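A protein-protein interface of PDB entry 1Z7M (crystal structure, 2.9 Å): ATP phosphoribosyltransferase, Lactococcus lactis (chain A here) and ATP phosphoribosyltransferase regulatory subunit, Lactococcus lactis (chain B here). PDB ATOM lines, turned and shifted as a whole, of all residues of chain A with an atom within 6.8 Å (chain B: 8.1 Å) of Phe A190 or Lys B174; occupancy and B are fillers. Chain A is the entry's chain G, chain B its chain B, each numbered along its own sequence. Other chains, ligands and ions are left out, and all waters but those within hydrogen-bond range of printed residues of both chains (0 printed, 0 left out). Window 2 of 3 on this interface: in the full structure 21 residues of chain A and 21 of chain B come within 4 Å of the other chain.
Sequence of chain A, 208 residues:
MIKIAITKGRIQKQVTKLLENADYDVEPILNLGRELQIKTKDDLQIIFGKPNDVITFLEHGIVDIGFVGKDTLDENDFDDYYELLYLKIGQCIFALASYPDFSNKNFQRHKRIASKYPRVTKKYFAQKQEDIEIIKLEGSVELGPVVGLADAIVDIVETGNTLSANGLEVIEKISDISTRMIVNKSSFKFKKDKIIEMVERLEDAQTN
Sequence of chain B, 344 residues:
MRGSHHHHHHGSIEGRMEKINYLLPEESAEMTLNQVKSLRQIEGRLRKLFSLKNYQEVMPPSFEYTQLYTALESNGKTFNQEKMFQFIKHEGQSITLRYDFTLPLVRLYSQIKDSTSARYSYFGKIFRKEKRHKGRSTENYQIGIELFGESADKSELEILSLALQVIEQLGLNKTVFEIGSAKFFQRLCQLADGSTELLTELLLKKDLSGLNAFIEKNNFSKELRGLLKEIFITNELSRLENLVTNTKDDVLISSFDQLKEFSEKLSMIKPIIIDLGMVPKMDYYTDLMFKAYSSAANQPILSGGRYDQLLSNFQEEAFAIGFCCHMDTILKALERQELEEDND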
ATOM      1  N   LYS A 185     -20.209  15.055  -9.995  1.00  0.00           N
ATOM      2  CA  LYS A 185     -19.127  14.075  -9.918  1.00  0.00           C
ATOM      3  C   LYS A 185     -19.543  12.812  -9.152  1.00  0.00           C
ATOM      4  O   LYS A 185     -19.148  11.698  -9.507  1.00  0.00           O
ATOM      5  CB  LYS A 185     -17.891  14.690  -9.235  1.00  0.00           C
ATOM      6  CG  LYS A 185     -17.130  15.747 -10.040  1.00  0.00           C
ATOM      7  CD  LYS A 185     -15.830  16.125  -9.342  1.00  0.00           C
ATOM      8  CE  LYS A 185     -15.165  17.299 -10.050  1.00  0.00           C
ATOM      9  NZ  LYS A 185     -13.958  17.859  -9.355  1.00  0.00           N
ATOM     10  N   SER A 186     -20.337  12.979  -8.101  1.00  0.00           N
ATOM     11  CA  SER A 186     -20.744  11.821  -7.344  1.00  0.00           C
ATOM     12  C   SER A 186     -21.742  11.024  -8.146  1.00  0.00           C
ATOM     13  O   SER A 186     -21.580   9.822  -8.322  1.00  0.00           O
ATOM     14  CB  SER A 186     -21.347  12.226  -6.012  1.00  0.00           C
ATOM     15  OG  SER A 186     -21.373  11.089  -5.151  1.00  0.00           O
ATOM     16  N   SER A 187     -22.773  11.696  -8.644  1.00  0.00           N
ATOM     17  CA  SER A 187     -23.784  11.016  -9.445  1.00  0.00           C
ATOM     18  C   SER A 187     -23.137  10.196 -10.566  1.00  0.00           C
ATOM     19  O   SER A 187     -23.564   9.082 -10.859  1.00  0.00           O
ATOM     20  CB  SER A 187     -24.766  12.018 -10.060  1.00  0.00           C
ATOM     21  OG  SER A 187     -25.542  12.656  -9.077  1.00  0.00           O
ATOM     22  N   PHE A 188     -22.102  10.742 -11.192  1.00  0.00           N
ATOM     23  CA  PHE A 188     -21.435  10.046 -12.282  1.00  0.00           C
ATOM     24  C   PHE A 188     -20.711   8.794 -11.800  1.00  0.00           C
ATOM     25  O   PHE A 188     -20.422   7.903 -12.588  1.00  0.00           O
ATOM     26  CB  PHE A 188     -20.439  10.985 -12.962  1.00  0.00           C
ATOM     27  CG  PHE A 188     -19.823  10.414 -14.198  1.00  0.00           C
ATOM     28  CD1 PHE A 188     -20.504  10.456 -15.412  1.00  0.00           C
ATOM     29  CD2 PHE A 188     -18.565   9.821 -14.148  1.00  0.00           C
ATOM     30  CE1 PHE A 188     -19.945   9.918 -16.556  1.00  0.00           C
ATOM     31  CE2 PHE A 188     -17.995   9.278 -15.284  1.00  0.00           C
ATOM     32  CZ  PHE A 188     -18.684   9.327 -16.494  1.00  0.00           C
ATOM     33  N   LYS A 189     -20.411   8.722 -10.508  1.00  0.00           N
ATOM     34  CA  LYS A 189     -19.706   7.558  -9.984  1.00  0.00           C
ATOM     35  C   LYS A 189     -20.661   6.467  -9.549  1.00  0.00           C
ATOM     36  O   LYS A 189     -20.278   5.299  -9.459  1.00  0.00           O
ATOM     37  CB  LYS A 189     -18.803   7.960  -8.815  1.00  0.00           C
ATOM     38  CG  LYS A 189     -17.886   9.135  -9.115  1.00  0.00           C
ATOM     39  CD  LYS A 189     -16.431   8.700  -9.170  1.00  0.00           C
ATOM     40  CE  LYS A 189     -15.514   9.875  -9.469  1.00  0.00           C
ATOM     41  NZ  LYS A 189     -14.085   9.463  -9.527  1.00  0.00           N
ATOM     42  N   PHE A 190     -21.910   6.836  -9.290  1.00  0.00           N
ATOM     43  CA  PHE A 190     -22.880   5.841  -8.869  1.00  0.00           C
ATOM     44  C   PHE A 190     -24.030   5.630  -9.835  1.00  0.00           C
ATOM     45  O   PHE A 190     -24.909   4.816  -9.590  1.00  0.00           O
ATOM     46  CB  PHE A 190     -23.403   6.157  -7.455  1.00  0.00           C
ATOM     47  CG  PHE A 190     -22.368   5.970  -6.383  1.00  0.00           C
ATOM     48  CD1 PHE A 190     -21.652   7.052  -5.892  1.00  0.00           C
ATOM     49  CD2 PHE A 190     -22.032   4.696  -5.945  1.00  0.00           C
ATOM     50  CE1 PHE A 190     -20.603   6.866  -4.986  1.00  0.00           C
ATOM     51  CE2 PHE A 190     -20.985   4.501  -5.041  1.00  0.00           C
ATOM     52  CZ  PHE A 190     -20.270   5.586  -4.564  1.00  0.00           C
ATOM     53  N   LYS A 191     -24.018   6.337 -10.948  1.00  0.00           N
ATOM     54  CA  LYS A 191     -25.076   6.179 -11.928  1.00  0.00           C
ATOM     55  C   LYS A 191     -24.516   6.359 -13.345  1.00  0.00           C
ATOM     56  O   LYS A 191     -25.224   6.793 -14.260  1.00  0.00           O
ATOM     57  CB  LYS A 191     -26.172   7.203 -11.654  1.00  0.00           C
ATOM     58  CG  LYS A 191     -26.701   7.207 -10.231  1.00  0.00           C
ATOM     59  CD  LYS A 191     -27.749   8.304 -10.124  1.00  0.00           C
ATOM     60  CE  LYS A 191     -28.417   8.385  -8.777  1.00  0.00           C
ATOM     61  NZ  LYS A 191     -29.440   9.455  -8.783  1.00  0.00           N
ATOM     62  N   LYS A 192     -23.239   6.008 -13.512  1.00  0.00           N
ATOM     63  CA  LYS A 192     -22.533   6.142 -14.792  1.00  0.00           C
ATOM     64  C   LYS A 192     -23.331   5.567 -15.945  1.00  0.00           C
ATOM     65  O   LYS A 192     -23.342   6.104 -17.056  1.00  0.00           O
ATOM     66  CB  LYS A 192     -21.173   5.452 -14.725  1.00  0.00           C
ATOM     67  CG  LYS A 192     -20.339   5.692 -15.955  1.00  0.00           C
ATOM     68  CD  LYS A 192     -18.920   5.205 -15.776  1.00  0.00           C
ATOM     69  CE  LYS A 192     -18.249   5.844 -14.584  1.00  0.00           C
ATOM     70  NZ  LYS A 192     -16.769   5.852 -14.748  1.00  0.00           N
ATOM     71  N   ASP A 193     -23.988   4.454 -15.670  1.00  0.00           N
ATOM     72  CA  ASP A 193     -24.819   3.803 -16.657  1.00  0.00           C
ATOM     73  C   ASP A 193     -25.710   4.827 -17.352  1.00  0.00           C
ATOM     74  O   ASP A 193     -25.343   5.397 -18.379  1.00  0.00           O
ATOM     75  CB  ASP A 193     -25.670   2.734 -15.961  1.00  0.00           C
ATOM     76  CG  ASP A 193     -26.141   3.171 -14.564  1.00  0.00           C
ATOM     77  OD1 ASP A 193     -27.145   3.924 -14.466  1.00  0.00           O
ATOM     78  OD2 ASP A 193     -25.490   2.763 -13.566  1.00  0.00           O
ATOM     79  N   ILE A 195     -26.215   7.737 -16.989  1.00  0.00           N
ATOM     80  CA  ILE A 195     -25.587   9.011 -17.303  1.00  0.00           C
ATOM     81  C   ILE A 195     -24.913   8.908 -18.662  1.00  0.00           C
ATOM     82  O   ILE A 195     -25.208   9.701 -19.556  1.00  0.00           O
ATOM     83  CB  ILE A 195     -24.541   9.446 -16.235  1.00  0.00           C
ATOM     84  CG1 ILE A 195     -25.191   9.558 -14.851  1.00  0.00           C
ATOM     85  CG2 ILE A 195     -23.955  10.820 -16.608  1.00  0.00           C
ATOM     86  CD1 ILE A 195     -26.061  10.772 -14.670  1.00  0.00           C
ATOM     87  N   ILE B 167     -12.143   2.890   5.837  1.00  0.00           N
ATOM     88  CA  ILE B 167     -13.447   3.061   5.237  1.00  0.00           C
ATOM     89  C   ILE B 167     -14.421   2.089   5.859  1.00  0.00           C
ATOM     90  O   ILE B 167     -15.630   2.339   5.894  1.00  0.00           O
ATOM     91  CB  ILE B 167     -13.372   2.832   3.759  1.00  0.00           C
ATOM     92  CG1 ILE B 167     -12.422   3.865   3.181  1.00  0.00           C
ATOM     93  CG2 ILE B 167     -14.741   2.928   3.139  1.00  0.00           C
ATOM     94  CD1 ILE B 167     -12.072   3.651   1.746  1.00  0.00           C
ATOM     95  N   GLY B 171     -19.439   4.332   9.157  1.00  0.00           N
ATOM     96  CA  GLY B 171     -20.649   3.580   8.880  1.00  0.00           C
ATOM     97  C   GLY B 171     -21.321   3.873   7.556  1.00  0.00           C
ATOM     98  O   GLY B 171     -22.547   3.973   7.498  1.00  0.00           O
ATOM     99  N   LEU B 172     -20.541   3.995   6.487  1.00  0.00           N
ATOM    100  CA  LEU B 172     -21.098   4.294   5.170  1.00  0.00           C
ATOM    101  C   LEU B 172     -21.418   3.032   4.376  1.00  0.00           C
ATOM    102  O   LEU B 172     -20.542   2.200   4.166  1.00  0.00           O
ATOM    103  CB  LEU B 172     -20.111   5.156   4.400  1.00  0.00           C
ATOM    104  CG  LEU B 172     -19.785   6.493   5.052  1.00  0.00           C
ATOM    105  CD1 LEU B 172     -18.636   7.129   4.316  1.00  0.00           C
ATOM    106  CD2 LEU B 172     -20.996   7.390   5.010  1.00  0.00           C
ATOM    107  N   ASN B 173     -22.664   2.910   3.915  1.00  0.00           N
ATOM    108  CA  ASN B 173     -23.113   1.732   3.162  1.00  0.00           C
ATOM    109  C   ASN B 173     -22.557   1.576   1.752  1.00  0.00           C
ATOM    110  O   ASN B 173     -21.911   0.577   1.456  1.00  0.00           O
ATOM    111  CB  ASN B 173     -24.638   1.691   3.077  1.00  0.00           C
ATOM    112  CG  ASN B 173     -25.306   1.957   4.404  1.00  0.00           C
ATOM    113  OD1 ASN B 173     -24.840   1.500   5.458  1.00  0.00           O
ATOM    114  ND2 ASN B 173     -26.422   2.691   4.365  1.00  0.00           N
ATOM    115  N   LYS B 174     -22.806   2.542   0.873  1.00  0.00           N
ATOM    116  CA  LYS B 174     -22.315   2.450  -0.504  1.00  0.00           C
ATOM    117  C   LYS B 174     -21.111   3.354  -0.837  1.00  0.00           C
ATOM    118  O   LYS B 174     -21.265   4.545  -1.130  1.00  0.00           O
ATOM    119  CB  LYS B 174     -23.465   2.737  -1.467  1.00  0.00           C
ATOM    120  CG  LYS B 174     -23.096   2.572  -2.928  1.00  0.00           C
ATOM    121  CD  LYS B 174     -24.326   2.670  -3.806  1.00  0.00           C
ATOM    122  CE  LYS B 174     -25.332   1.590  -3.424  1.00  0.00           C
ATOM    123  NZ  LYS B 174     -26.601   1.691  -4.198  1.00  0.00           N
ATOM    124  N   THR B 175     -19.915   2.770  -0.806  1.00  0.00           N
ATOM    125  CA  THR B 175     -18.692   3.522  -1.092  1.00  0.00           C
ATOM    126  C   THR B 175     -17.735   2.848  -2.065  1.00  0.00           C
ATOM    127  O   THR B 175     -17.414   1.667  -1.930  1.00  0.00           O
ATOM    128  CB  THR B 175     -17.853   3.804   0.189  1.00  0.00           C
ATOM    129  OG1 THR B 175     -17.330   2.574   0.714  1.00  0.00           O
ATOM    130  CG2 THR B 175     -18.693   4.493   1.246  1.00  0.00           C
ATOM    131  N   VAL B 176     -17.250   3.618  -3.028  1.00  0.00           N
ATOM    132  CA  VAL B 176     -16.299   3.101  -3.991  1.00  0.00           C
ATOM    133  C   VAL B 176     -14.909   3.684  -3.751  1.00  0.00           C
ATOM    134  O   VAL B 176     -14.750   4.851  -3.383  1.00  0.00           O
ATOM    135  CB  VAL B 176     -16.735   3.412  -5.432  1.00  0.00           C
ATOM    136  CG1 VAL B 176     -18.163   2.953  -5.631  1.00  0.00           C
ATOM    137  CG2 VAL B 176     -16.594   4.892  -5.724  1.00  0.00           C
ATOM    138  N   PHE B 177     -13.908   2.845  -3.960  1.00  0.00           N
ATOM    139  CA  PHE B 177     -12.524   3.232  -3.786  1.00  0.00           C
ATOM    140  C   PHE B 177     -11.877   3.233  -5.180  1.00  0.00           C
ATOM    141  O   PHE B 177     -12.064   2.285  -5.946  1.00  0.00           O
ATOM    142  CB  PHE B 177     -11.855   2.219  -2.874  1.00  0.00           C
ATOM    143  CG  PHE B 177     -10.510   2.621  -2.435  1.00  0.00           C
ATOM    144  CD1 PHE B 177     -10.343   3.365  -1.281  1.00  0.00           C
ATOM    145  CD2 PHE B 177      -9.395   2.251  -3.171  1.00  0.00           C
ATOM    146  CE1 PHE B 177      -9.074   3.739  -0.857  1.00  0.00           C
ATOM    147  CE2 PHE B 177      -8.119   2.616  -2.764  1.00  0.00           C
ATOM    148  CZ  PHE B 177      -7.955   3.361  -1.601  1.00  0.00           C
ATOM    149  N   GLU B 178     -11.138   4.291  -5.512  1.00  0.00           N
ATOM    150  CA  GLU B 178     -10.492   4.423  -6.830  1.00  0.00           C
ATOM    151  C   GLU B 178      -8.994   4.654  -6.765  1.00  0.00           C
ATOM    152  O   GLU B 178      -8.534   5.538  -6.049  1.00  0.00           O
ATOM    153  CB  GLU B 178     -11.086   5.594  -7.616  1.00  0.00           C
ATOM    154  CG  GLU B 178     -12.533   5.437  -8.042  1.00  0.00           C
ATOM    155  CD  GLU B 178     -13.107   6.729  -8.621  1.00  0.00           C
ATOM    156  OE1 GLU B 178     -14.285   6.724  -9.043  1.00  0.00           O
ATOM    157  OE2 GLU B 178     -12.387   7.755  -8.647  1.00  0.00           O
ATOM    158  N   LYS B 270     -11.866  -5.293  -0.403  1.00  0.00           N
ATOM    159  CA  LYS B 270     -12.924  -4.512  -1.041  1.00  0.00           C
ATOM    160  C   LYS B 270     -12.653  -4.400  -2.536  1.00  0.00           C
ATOM    161  O   LYS B 270     -11.503  -4.300  -2.960  1.00  0.00           O
ATOM    162  CB  LYS B 270     -12.977  -3.110  -0.447  1.00  0.00           C
ATOM    163  CG  LYS B 270     -14.038  -2.220  -1.067  1.00  0.00           C
ATOM    164  CD  LYS B 270     -14.050  -0.844  -0.422  1.00  0.00           C
ATOM    165  CE  LYS B 270     -15.249  -0.042  -0.877  1.00  0.00           C
ATOM    166  NZ  LYS B 270     -16.513  -0.707  -0.471  1.00  0.00           N
ATOM    167  N   ILE B 273     -11.307  -0.025  -7.711  1.00  0.00           N
ATOM    168  CA  ILE B 273     -11.638   0.467  -9.029  1.00  0.00           C
ATOM    169  C   ILE B 273     -10.453   1.228  -9.608  1.00  0.00           C
ATOM    170  O   ILE B 273      -9.848   2.067  -8.947  1.00  0.00           O
ATOM    171  CB  ILE B 273     -12.871   1.341  -8.953  1.00  0.00           C
ATOM    172  CG1 ILE B 273     -14.058   0.466  -8.578  1.00  0.00           C
ATOM    173  CG2 ILE B 273     -13.113   2.019 -10.256  1.00  0.00           C
ATOM    174  CD1 ILE B 273     -15.285   1.242  -8.184  1.00  0.00           C
ATOM    175  N   ALA B 292     -11.935   8.093  -2.632  1.00  0.00           N
ATOM    176  CA  ALA B 292     -12.994   7.233  -2.132  1.00  0.00           C
ATOM    177  C   ALA B 292     -14.242   8.076  -2.015  1.00  0.00           C
ATOM    178  O   ALA B 292     -14.202   9.153  -1.430  1.00  0.00           O
ATOM    179  CB  ALA B 292     -12.615   6.670  -0.775  1.00  0.00           C
ATOM    180  N   TYR B 293     -15.347   7.590  -2.573  1.00  0.00           N
ATOM    181  CA  TYR B 293     -16.602   8.331  -2.531  1.00  0.00           C
ATOM    182  C   TYR B 293     -17.731   7.560  -1.860  1.00  0.00           C
ATOM    183  O   TYR B 293     -17.666   6.341  -1.725  1.00  0.00           O
ATOM    184  CB  TYR B 293     -17.047   8.713  -3.943  1.00  0.00           C
ATOM    185  CG  TYR B 293     -16.153   9.716  -4.628  1.00  0.00           C
ATOM    186  CD1 TYR B 293     -14.887   9.354  -5.086  1.00  0.00           C
ATOM    187  CD2 TYR B 293     -16.566  11.034  -4.805  1.00  0.00           C
ATOM    188  CE1 TYR B 293     -14.049  10.284  -5.702  1.00  0.00           C
ATOM    189  CE2 TYR B 293     -15.739  11.976  -5.420  1.00  0.00           C
ATOM    190  CZ  TYR B 293     -14.482  11.598  -5.862  1.00  0.00           C
ATOM    191  OH  TYR B 293     -13.642  12.533  -6.432  1.00  0.00           O
ATOM    192  N   SER B 294     -18.755   8.291  -1.428  1.00  0.00           N
ATOM    193  CA  SER B 294     -19.938   7.707  -0.798  1.00  0.00           C
ATOM    194  C   SER B 294     -21.111   8.166  -1.623  1.00  0.00           C
ATOM    195  O   SER B 294     -21.177   9.335  -2.002  1.00  0.00           O
ATOM    196  CB  SER B 294     -20.133   8.215   0.637  1.00  0.00           C
ATOM    197  OG  SER B 294     -21.501   8.106   1.035  1.00  0.00           O
ATOM    198  N   SER B 295     -22.038   7.262  -1.907  1.00  0.00           N
ATOM    199  CA  SER B 295     -23.198   7.642  -2.696  1.00  0.00           C
ATOM    200  C   SER B 295     -23.954   8.745  -1.982  1.00  0.00           C
ATOM    201  O   SER B 295     -24.817   9.382  -2.569  1.00  0.00           O
ATOM    202  CB  SER B 295     -24.121   6.441  -2.901  1.00  0.00           C
ATOM    203  OG  SER B 295     -24.403   5.795  -1.667  1.00  0.00           O
ATOM    204  N   ALA B 296     -23.605   8.982  -0.720  1.00  0.00           N
ATOM    205  CA  ALA B 296     -24.277   9.997   0.088  1.00  0.00           C
ATOM    206  C   ALA B 296     -23.606  11.375   0.162  1.00  0.00           C
ATOM    207  O   ALA B 296     -23.991  12.213   0.978  1.00  0.00           O
ATOM    208  CB  ALA B 296     -24.496   9.456   1.494  1.00  0.00           C
ATOM    209  N   ALA B 297     -22.606  11.616  -0.675  1.00  0.00           N
ATOM    210  CA  ALA B 297     -21.931  12.906  -0.688  1.00  0.00           C
ATOM    211  C   ALA B 297     -21.315  13.136  -2.057  1.00  0.00           C
ATOM    212  O   ALA B 297     -20.989  12.188  -2.773  1.00  0.00           O
ATOM    213  CB  ALA B 297     -20.871  12.955   0.380  1.00  0.00           C
ATOM    214  N   ASN B 298     -21.130  14.403  -2.403  1.00  0.00           N
ATOM    215  CA  ASN B 298     -20.597  14.777  -3.704  1.00  0.00           C
ATOM    216  C   ASN B 298     -19.087  14.942  -3.670  1.00  0.00           C
ATOM    217  O   ASN B 298     -18.418  15.031  -4.704  1.00  0.00           O
ATOM    218  CB  ASN B 298     -21.254  16.081  -4.133  1.00  0.00           C
ATOM    219  CG  ASN B 298     -22.700  16.171  -3.683  1.00  0.00           C
ATOM    220  OD1 ASN B 298     -23.573  15.467  -4.197  1.00  0.00           O
ATOM    221  ND2 ASN B 298     -22.955  17.019  -2.699  1.00  0.00           N
ATOM    222  N   GLN B 299     -18.550  14.980  -2.468  1.00  0.00           N
ATOM    223  CA  GLN B 299     -17.131  15.137  -2.309  1.00  0.00           C
ATOM    224  C   GLN B 299     -16.508  13.824  -1.891  1.00  0.00           C
ATOM    225  O   GLN B 299     -17.204  12.918  -1.421  1.00  0.00           O
ATOM    226  CB  GLN B 299     -16.883  16.213  -1.264  1.00  0.00           C
ATOM    227  CG  GLN B 299     -17.154  17.599  -1.778  1.00  0.00           C
ATOM    228  CD  GLN B 299     -15.864  18.249  -2.256  1.00  0.00           C
ATOM    229  N   ILE B 301     -14.689  11.127   0.374  1.00  0.00           N
ATOM    230  CA  ILE B 301     -14.626  10.959   1.817  1.00  0.00           C
ATOM    231  C   ILE B 301     -13.172  10.748   2.227  1.00  0.00           C
ATOM    232  O   ILE B 301     -12.776  11.027   3.354  1.00  0.00           O
ATOM    233  CB  ILE B 301     -15.489   9.759   2.296  1.00  0.00           C
ATOM    234  CG1 ILE B 301     -15.117   8.492   1.528  1.00  0.00           C
ATOM    235  CG2 ILE B 301     -16.960  10.092   2.135  1.00  0.00           C
ATOM    236  CD1 ILE B 301     -15.960   7.291   1.874  1.00  0.00           C
ATOM    237  N   ALA B 333     -22.570  12.730   4.977  1.00  0.00           N
ATOM    238  CA  ALA B 333     -23.021  11.551   4.238  1.00  0.00           C
ATOM    239  C   ALA B 333     -23.725  10.565   5.155  1.00  0.00           C
ATOM    240  O   ALA B 333     -24.674   9.904   4.745  1.00  0.00           O
ATOM    241  CB  ALA B 333     -21.846  10.870   3.553  1.00  0.00           C
ATOM    242  N   GLN B 337     -27.537   9.470   4.408  1.00  0.00           N
ATOM    243  CA  GLN B 337     -27.688   8.019   4.379  1.00  0.00           C
ATOM    244  C   GLN B 337     -28.797   7.523   5.312  1.00  0.00           C
ATOM    245  O   GLN B 337     -29.581   6.636   4.955  1.00  0.00           O
ATOM    246  CB  GLN B 337     -26.360   7.370   4.770  1.00  0.00           C
ATOM    247  CG  GLN B 337     -26.253   5.887   4.480  1.00  0.00           C
ATOM    248  CD  GLN B 337     -24.923   5.301   4.936  1.00  0.00           C
ATOM    249  OE1 GLN B 337     -24.658   5.184   6.129  1.00  0.00           O
ATOM    250  NE2 GLN B 337     -24.074   4.944   3.981  1.00  0.00           N
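Of chain B, only Lys B174, Val B176, Tyr B293, Ser B294 and Ser B295 come within 4 Å of Phe A190. Lys B174 touches just one residue of chain A: Phe A190 (3.6 Å). Printed residues of chain A within 4 Å of Glu B178: Lys A189 (2.6 Å). Of the printed residues of chain A, Tyr B293 touches Lys A189 and Phe A190. Of the printed residues of chain A, Asn B298 touches Ser A186. The nearest printed residue of chain A that does not touch Lys B174 is Lys A189 (7.4 Å). The nearest printed residue of chain A that does not touch Tyr B293 is Ser A186 (4.8 Å).
Among the printed residues, merely in contact across the chains: Phe A190 with Val B176, Phe A190 with Ser B295, Ser A186 with Asn B298, Phe A190 with Lys B174, Ser A186 with Ser B294, Phe A190 with Ser B294, Lys A189 with Tyr B293 and Phe A190 with Tyr B293.
The backbone carbonyl oxygen (O) of Lys B174 sits at hydrogen-bond distance from the backbone NH (N) of Ser B295 (2.9 Å). O of Val B176 lies within hydrogen-bond range of N of Tyr B293 (2.9 Å). OG of Ser B294 lies close to N of Ala B296.
Of the 22 printed residues of chain B, 8 touch a printed residue of chain A. Hydrophobic or aromatic side chains of chain B that line the printed part of chain A: Val B176 and Tyr B293. Of the 10 printed residues of chain A, 3 touch a printed residue of chain B. Hydrophobic or aromatic side chains of chain A that line the printed part of chain B: Phe A190. Among the printed residues, Asp or Glu carboxylates within 4 Å of a Lys or Arg side-chain nitrogen of the other chain: Lys A189 with Glu B178 (2.6 Å).
NZ of Lys A189 lies within salt-bridge range of OE2 of Glu B178. O of Ala B297 lies within hydrogen-bond range of OG of Ser A186 (2.6 Å).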
